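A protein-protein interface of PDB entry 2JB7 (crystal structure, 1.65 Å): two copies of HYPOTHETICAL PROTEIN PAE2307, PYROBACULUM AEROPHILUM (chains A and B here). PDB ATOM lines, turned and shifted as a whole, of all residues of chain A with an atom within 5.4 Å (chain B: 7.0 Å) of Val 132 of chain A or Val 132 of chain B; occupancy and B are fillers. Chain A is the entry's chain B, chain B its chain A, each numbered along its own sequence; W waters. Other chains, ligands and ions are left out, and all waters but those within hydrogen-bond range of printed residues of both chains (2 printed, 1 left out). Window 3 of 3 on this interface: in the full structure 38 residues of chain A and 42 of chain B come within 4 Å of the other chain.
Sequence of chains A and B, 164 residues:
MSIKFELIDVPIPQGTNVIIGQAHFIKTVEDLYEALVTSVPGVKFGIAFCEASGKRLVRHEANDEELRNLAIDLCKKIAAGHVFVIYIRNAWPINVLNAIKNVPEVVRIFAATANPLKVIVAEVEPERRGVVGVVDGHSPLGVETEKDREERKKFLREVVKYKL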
ATOM      1  N   PHE A   5       9.984 -17.134   4.095  1.00  0.00           N
ATOM      2  CA  PHE A   5       8.622 -17.288   3.575  1.00  0.00           C
ATOM      3  C   PHE A   5       8.632 -18.394   2.512  1.00  0.00           C
ATOM      4  O   PHE A   5       9.558 -18.448   1.697  1.00  0.00           O
ATOM      5  CB  PHE A   5       8.121 -15.966   3.006  1.00  0.00           C
ATOM      6  CG  PHE A   5       7.972 -14.883   4.034  1.00  0.00           C
ATOM      7  CD1 PHE A   5       6.897 -14.885   4.915  1.00  0.00           C
ATOM      8  CD2 PHE A   5       8.900 -13.872   4.136  1.00  0.00           C
ATOM      9  CE1 PHE A   5       6.751 -13.881   5.877  1.00  0.00           C
ATOM     10  CE2 PHE A   5       8.760 -12.864   5.100  1.00  0.00           C
ATOM     11  CZ  PHE A   5       7.678 -12.877   5.968  1.00  0.00           C
ATOM     12  N   ILE A 120       0.790 -18.972   2.151  1.00  0.00           N
ATOM     13  CA  ILE A 120       2.075 -18.351   2.454  1.00  0.00           C
ATOM     14  C   ILE A 120       2.426 -18.753   3.879  1.00  0.00           C
ATOM     15  O   ILE A 120       1.652 -18.513   4.806  1.00  0.00           O
ATOM     16  CB  ILE A 120       2.047 -16.820   2.353  1.00  0.00           C
ATOM     17  CG1 ILE A 120       1.597 -16.350   0.943  1.00  0.00           C
ATOM     18  CG2 ILE A 120       3.434 -16.294   2.607  1.00  0.00           C
ATOM     19  CD1 ILE A 120       1.306 -14.859   0.861  1.00  0.00           C
ATOM     20  N   VAL A 121       3.562 -19.420   4.049  1.00  0.00           N
ATOM     21  CA  VAL A 121       3.973 -19.924   5.359  1.00  0.00           C
ATOM     22  C   VAL A 121       5.288 -19.256   5.747  1.00  0.00           C
ATOM     23  O   VAL A 121       6.209 -19.129   4.915  1.00  0.00           O
ATOM     24  CB  VAL A 121       4.142 -21.477   5.373  1.00  0.00           C
ATOM     25  CG1 VAL A 121       4.684 -21.972   6.700  1.00  0.00           C
ATOM     26  CG2 VAL A 121       2.801 -22.152   5.046  1.00  0.00           C
ATOM     27  N   ALA A 122       5.364 -18.787   6.990  1.00  0.00           N
ATOM     28  CA  ALA A 122       6.610 -18.287   7.559  1.00  0.00           C
ATOM     29  C   ALA A 122       7.255 -19.377   8.379  1.00  0.00           C
ATOM     30  O   ALA A 122       6.595 -20.020   9.176  1.00  0.00           O
ATOM     31  CB  ALA A 122       6.380 -17.072   8.423  1.00  0.00           C
ATOM     32  N   GLY A 130       4.243 -20.865  10.773  1.00  0.00           N
ATOM     33  CA  GLY A 130       2.926 -20.246  10.896  1.00  0.00           C
ATOM     34  C   GLY A 130       2.424 -19.793   9.539  1.00  0.00           C
ATOM     35  O   GLY A 130       3.200 -19.461   8.650  1.00  0.00           O
ATOM     36  N   VAL A 131       1.102 -19.765   9.386  1.00  0.00           N
ATOM     37  CA  VAL A 131       0.475 -19.245   8.183  1.00  0.00           C
ATOM     38  C   VAL A 131       0.364 -17.726   8.214  1.00  0.00           C
ATOM     39  O   VAL A 131      -0.188 -17.141   9.167  1.00  0.00           O
ATOM     40  CB  VAL A 131      -0.908 -19.895   7.958  1.00  0.00           C
ATOM     41  CG1 VAL A 131      -1.672 -19.180   6.811  1.00  0.00           C
ATOM     42  CG2 VAL A 131      -0.769 -21.418   7.699  1.00  0.00           C
ATOM     43  N   VAL A 132       0.886 -17.089   7.173  1.00  0.00           N
ATOM     44  CA  VAL A 132       0.878 -15.652   7.065  1.00  0.00           C
ATOM     45  C   VAL A 132      -0.351 -15.177   6.286  1.00  0.00           C
ATOM     46  O   VAL A 132      -0.969 -14.193   6.639  1.00  0.00           O
ATOM     47  CB  VAL A 132       2.138 -15.147   6.406  1.00  0.00           C
ATOM     48  CG1 VAL A 132       1.953 -13.715   5.884  1.00  0.00           C
ATOM     49  CG2 VAL A 132       3.300 -15.226   7.418  1.00  0.00           C
ATOM     50  N   GLY A 133      -0.718 -15.920   5.259  1.00  0.00           N
ATOM     51  CA  GLY A 133      -1.844 -15.535   4.438  1.00  0.00           C
ATOM     52  C   GLY A 133      -2.057 -16.541   3.348  1.00  0.00           C
ATOM     53  O   GLY A 133      -1.411 -17.598   3.314  1.00  0.00           O
ATOM     54  N   VAL A 134      -2.966 -16.203   2.447  1.00  0.00           N
ATOM     55  CA  VAL A 134      -3.268 -17.048   1.303  1.00  0.00           C
ATOM     56  C   VAL A 134      -3.440 -16.173   0.062  1.00  0.00           C
ATOM     57  O   VAL A 134      -3.638 -14.953   0.151  1.00  0.00           O
ATOM     58  CB  VAL A 134      -4.583 -17.867   1.496  1.00  0.00           C
ATOM     59  CG1 VAL A 134      -4.494 -18.799   2.736  1.00  0.00           C
ATOM     60  CG2 VAL A 134      -5.826 -16.925   1.551  1.00  0.00           C
ATOM     61  N   ILE B   3       8.465 -13.544  -3.320  1.00  0.00           N
ATOM     62  CA  ILE B   3       7.302 -12.818  -2.790  1.00  0.00           C
ATOM     63  C   ILE B   3       7.564 -11.311  -2.690  1.00  0.00           C
ATOM     64  O   ILE B   3       8.542 -10.878  -2.085  1.00  0.00           O
ATOM     65  CB  ILE B   3       6.896 -13.307  -1.396  1.00  0.00           C
ATOM     66  CG1 ILE B   3       6.631 -14.821  -1.386  1.00  0.00           C
ATOM     67  CG2 ILE B   3       5.651 -12.548  -0.927  1.00  0.00           C
ATOM     68  CD1 ILE B   3       6.285 -15.358   0.031  1.00  0.00           C
ATOM     69  N   LYS B   4       6.677 -10.505  -3.280  1.00  0.00           N
ATOM     70  CA  LYS B   4       6.767  -9.064  -3.208  1.00  0.00           C
ATOM     71  C   LYS B   4       5.692  -8.585  -2.235  1.00  0.00           C
ATOM     72  O   LYS B   4       4.539  -8.991  -2.353  1.00  0.00           O
ATOM     73  CB  LYS B   4       6.549  -8.440  -4.585  1.00  0.00           C
ATOM     74  N   PHE B   5       6.088  -7.751  -1.280  1.00  0.00           N
ATOM     75  CA  PHE B   5       5.163  -7.106  -0.358  1.00  0.00           C
ATOM     76  C   PHE B   5       4.930  -5.699  -0.824  1.00  0.00           C
ATOM     77  O   PHE B   5       5.849  -5.012  -1.286  1.00  0.00           O
ATOM     78  CB  PHE B   5       5.695  -7.134   1.074  1.00  0.00           C
ATOM     79  CG  PHE B   5       5.889  -8.515   1.604  1.00  0.00           C
ATOM     80  CD1 PHE B   5       4.816  -9.250   2.052  1.00  0.00           C
ATOM     81  CD2 PHE B   5       7.150  -9.083   1.663  1.00  0.00           C
ATOM     82  CE1 PHE B   5       4.964 -10.498   2.532  1.00  0.00           C
ATOM     83  CE2 PHE B   5       7.322 -10.360   2.158  1.00  0.00           C
ATOM     84  CZ  PHE B   5       6.245 -11.076   2.606  1.00  0.00           C
ATOM     85  N   ARG B 108     -13.135 -14.303   6.886  1.00  0.00           N
ATOM     86  CA  ARG B 108     -12.381 -13.544   7.869  1.00  0.00           C
ATOM     87  C   ARG B 108     -12.575 -12.044   7.678  1.00  0.00           C
ATOM     88  O   ARG B 108     -12.943 -11.570   6.594  1.00  0.00           O
ATOM     89  CB  ARG B 108     -10.901 -13.874   7.770  1.00  0.00           C
ATOM     90  CG  ARG B 108     -10.321 -13.586   6.395  1.00  0.00           C
ATOM     91  CD  ARG B 108      -9.278 -14.617   5.905  1.00  0.00           C
ATOM     92  NE  ARG B 108      -8.044 -14.516   6.685  1.00  0.00           N
ATOM     93  CZ  ARG B 108      -6.823 -14.431   6.167  1.00  0.00           C
ATOM     94  NH1 ARG B 108      -6.597 -14.497   4.838  1.00  0.00           N
ATOM     95  NH2 ARG B 108      -5.812 -14.291   6.996  1.00  0.00           N
ATOM     96  N   PHE B 110     -10.306  -8.476   8.356  1.00  0.00           N
ATOM     97  CA  PHE B 110      -8.954  -7.983   8.654  1.00  0.00           C
ATOM     98  C   PHE B 110      -8.920  -6.741   9.508  1.00  0.00           C
ATOM     99  O   PHE B 110      -7.982  -6.572  10.264  1.00  0.00           O
ATOM    100  CB  PHE B 110      -8.188  -7.669   7.366  1.00  0.00           C
ATOM    101  CG  PHE B 110      -8.033  -8.839   6.425  1.00  0.00           C
ATOM    102  CD1 PHE B 110      -7.238  -9.915   6.772  1.00  0.00           C
ATOM    103  CD2 PHE B 110      -8.687  -8.849   5.198  1.00  0.00           C
ATOM    104  CE1 PHE B 110      -7.066 -11.015   5.924  1.00  0.00           C
ATOM    105  CE2 PHE B 110      -8.539  -9.944   4.324  1.00  0.00           C
ATOM    106  CZ  PHE B 110      -7.730 -11.015   4.679  1.00  0.00           C
ATOM    107  N   VAL B 119      -2.888  -1.685   4.336  1.00  0.00           N
ATOM    108  CA  VAL B 119      -3.083  -3.098   4.054  1.00  0.00           C
ATOM    109  C   VAL B 119      -1.786  -3.609   3.471  1.00  0.00           C
ATOM    110  O   VAL B 119      -1.190  -2.967   2.611  1.00  0.00           O
ATOM    111  CB  VAL B 119      -4.239  -3.347   3.065  1.00  0.00           C
ATOM    112  CG1 VAL B 119      -4.366  -4.836   2.747  1.00  0.00           C
ATOM    113  CG2 VAL B 119      -5.574  -2.807   3.645  1.00  0.00           C
ATOM    114  N   ILE B 120      -1.306  -4.717   4.008  1.00  0.00           N
ATOM    115  CA  ILE B 120      -0.114  -5.355   3.532  1.00  0.00           C
ATOM    116  C   ILE B 120      -0.510  -6.462   2.584  1.00  0.00           C
ATOM    117  O   ILE B 120      -1.192  -7.385   2.978  1.00  0.00           O
ATOM    118  CB  ILE B 120       0.734  -5.933   4.687  1.00  0.00           C
ATOM    119  CG1 ILE B 120       1.026  -4.850   5.739  1.00  0.00           C
ATOM    120  CG2 ILE B 120       2.031  -6.448   4.148  1.00  0.00           C
ATOM    121  CD1 ILE B 120       1.744  -5.368   7.012  1.00  0.00           C
ATOM    122  N   VAL B 121      -0.078  -6.357   1.329  1.00  0.00           N
ATOM    123  CA  VAL B 121      -0.451  -7.341   0.280  1.00  0.00           C
ATOM    124  C   VAL B 121       0.841  -8.052  -0.206  1.00  0.00           C
ATOM    125  O   VAL B 121       1.883  -7.383  -0.362  1.00  0.00           O
ATOM    126  CB  VAL B 121      -1.132  -6.653  -0.901  1.00  0.00           C
ATOM    127  CG1 VAL B 121      -1.488  -7.634  -2.017  1.00  0.00           C
ATOM    128  CG2 VAL B 121      -2.409  -5.931  -0.430  1.00  0.00           C
ATOM    129  N   ALA B 122       0.726  -9.358  -0.437  1.00  0.00           N
ATOM    130  CA  ALA B 122       1.759 -10.189  -1.030  1.00  0.00           C
ATOM    131  C   ALA B 122       1.361 -10.495  -2.445  1.00  0.00           C
ATOM    132  O   ALA B 122       0.236 -10.935  -2.695  1.00  0.00           O
ATOM    133  CB  ALA B 122       1.892 -11.479  -0.276  1.00  0.00           C
ATOM    134  N   GLU B 123       2.275 -10.240  -3.366  1.00  0.00           N
ATOM    135  CA  GLU B 123       2.142 -10.706  -4.738  1.00  0.00           C
ATOM    136  C   GLU B 123       3.192 -11.790  -4.945  1.00  0.00           C
ATOM    137  O   GLU B 123       4.386 -11.546  -4.788  1.00  0.00           O
ATOM    138  CB  GLU B 123       2.355  -9.562  -5.714  1.00  0.00           C
ATOM    139  CG  GLU B 123       2.094  -9.973  -7.141  1.00  0.00           C
ATOM    140  CD  GLU B 123       2.082  -8.815  -8.113  1.00  0.00           C
ATOM    141  OE1 GLU B 123       1.425  -7.804  -7.844  1.00  0.00           O
ATOM    142  OE2 GLU B 123       2.732  -8.930  -9.182  1.00  0.00           O
ATOM    143  N   GLY B 130      -2.498 -11.669  -2.195  1.00  0.00           N
ATOM    144  CA  GLY B 130      -3.271 -11.952  -0.996  1.00  0.00           C
ATOM    145  C   GLY B 130      -2.931 -10.997   0.117  1.00  0.00           C
ATOM    146  O   GLY B 130      -1.867 -10.385   0.154  1.00  0.00           O
ATOM    147  N   VAL B 131      -3.872 -10.855   1.037  1.00  0.00           N
ATOM    148  CA  VAL B 131      -3.659  -9.988   2.175  1.00  0.00           C
ATOM    149  C   VAL B 131      -2.822 -10.689   3.277  1.00  0.00           C
ATOM    150  O   VAL B 131      -3.192 -11.728   3.753  1.00  0.00           O
ATOM    151  CB  VAL B 131      -4.982  -9.504   2.745  1.00  0.00           C
ATOM    152  CG1 VAL B 131      -4.708  -8.618   3.956  1.00  0.00           C
ATOM    153  CG2 VAL B 131      -5.739  -8.736   1.683  1.00  0.00           C
ATOM    154  N   VAL B 132      -1.752 -10.026   3.686  1.00  0.00           N
ATOM    155  CA  VAL B 132      -0.827 -10.494   4.713  1.00  0.00           C
ATOM    156  C   VAL B 132      -1.240  -9.936   6.062  1.00  0.00           C
ATOM    157  O   VAL B 132      -1.079 -10.600   7.084  1.00  0.00           O
ATOM    158  CB  VAL B 132       0.628 -10.067   4.347  1.00  0.00           C
ATOM    159  CG1 VAL B 132       1.599 -10.186   5.526  1.00  0.00           C
ATOM    160  CG2 VAL B 132       1.095 -10.909   3.177  1.00  0.00           C
ATOM    161  N   GLY B 133      -1.760  -8.737   6.087  1.00  0.00           N
ATOM    162  CA  GLY B 133      -2.189  -8.151   7.341  1.00  0.00           C
ATOM    163  C   GLY B 133      -2.531  -6.709   7.159  1.00  0.00           C
ATOM    164  O   GLY B 133      -2.629  -6.226   6.026  1.00  0.00           O
ATOM    165  N   VAL B 134      -2.775  -6.027   8.274  1.00  0.00           N
ATOM    166  CA  VAL B 134      -3.066  -4.610   8.242  1.00  0.00           C
ATOM    167  C   VAL B 134      -2.281  -3.916   9.343  1.00  0.00           C
ATOM    168  O   VAL B 134      -1.798  -4.533  10.288  1.00  0.00           O
ATOM    169  CB  VAL B 134      -4.568  -4.292   8.430  1.00  0.00           C
ATOM    170  CG1 VAL B 134      -5.406  -4.921   7.316  1.00  0.00           C
ATOM    171  CG2 VAL B 134      -5.027  -4.765   9.797  1.00  0.00           C
HETATM  172  O   HOH W   1      -4.602 -13.894   2.861  1.00  0.00           O
HETATM  173  O   HOH W   2      -6.203 -12.835   0.766  1.00  0.00           O
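Hydrophobic or aromatic side chains of chain B that line the printed part of chain A: Ile 3, Phe 5, Ala 122 and Val 132.
Along chain B the printed residues that touch a printed residue of chain A span positions 3 to 132.
Hydrophobic or aromatic side chains of chain A within 4 Å of the printed part of chain B: Phe 5, Ile 120 and Val 132.
Among the printed residues, no Asp or Glu carboxylate lies within 4 Å of a Lys or Arg side-chain nitrogen of the other chain.
Phe 5 of chain A touches its own counterpart, Phe 5 of chain B.
Ile 120 of chain A touches Ala 122 of chain B, but with the chains exchanged Ala 122 of chain A does not touch Ile 120 of chain B (12.2 Å).
Val 132 of chain A touches its own counterpart, Val 132 of chain B.
Val 134 of chain A touches Gly 130 of chain B, but with the chains exchanged Gly 130 of chain A does not touch Val 134 of chain B (14.7 Å).
9 positions are printed for both chains.
Of the 6 pairs that touch across the chains among the printed residues, 2 have their exchanged pair printed and touching as well.
Printed residues of chain B within 4 Å of Ile 120 of chain A: Ile 3 (3.95 Å) and Ala 122 (3.6 Å).
Of chain B, only Val 132 comes within 4 Å of Val 132 of chain A.
Printed residues of chain B within 4 Å of Val 134 of chain A: Gly 130.
Of the printed residues of chain A, Gly 130 of chain B touches Val 134.
Of chain A, only Val 132 comes within 4 Å of Val 132 of chain B.
The nearest residue of chain A that does not touch Val 132 of chain B is Ile 120 of chain A (4.6 Å).
Water W1 lies within hydrogen-bond range of O of Val 131 of chain B, N of Val 134 of chain A and NH1 of Arg 108 of chain B.
Water W2 bridges N of Val 131 of chain B (3.1 Å) and O of Val 134 of chain A (3.4 Å).
O of Gly 130 of chain B sits at hydrogen-bond distance from N of Ala 122 of chain B (2.9 Å).
N of Val 132 of chain A is in hydrogen-bond range of O of Ile 120 of chain A (2.9 Å).
The backbone NH (N) of Ile 120 of chain A sits at hydrogen-bond distance from the backbone carbonyl oxygen (O) of Gly 133 of chain A (2.8 Å).
The backbone NH of Val 132 of chain B is in hydrogen-bond range of the backbone carbonyl oxygen of Ile 120 of chain B, 2.8 Å away.
Ile 3 of chain B touches Phe 5 of chain A.
CZ of Phe 5 of chain B touches CE2 of Phe 5 of chain A, at 3.97 Å.
Ile 3 of chain B touches Ile 120 of chain A (CD1 to CG2, 3.95 Å).
Ile 120 of chain A touches Ala 122 of chain B (CD1 to CB, 3.6 Å).
Val 132 of chain A touches Val 132 of chain B (CG1 to CG1, 3.6 Å).
Gly 130 of chain B touches Val 134 of chain A (CA to O, 3.2 Å).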
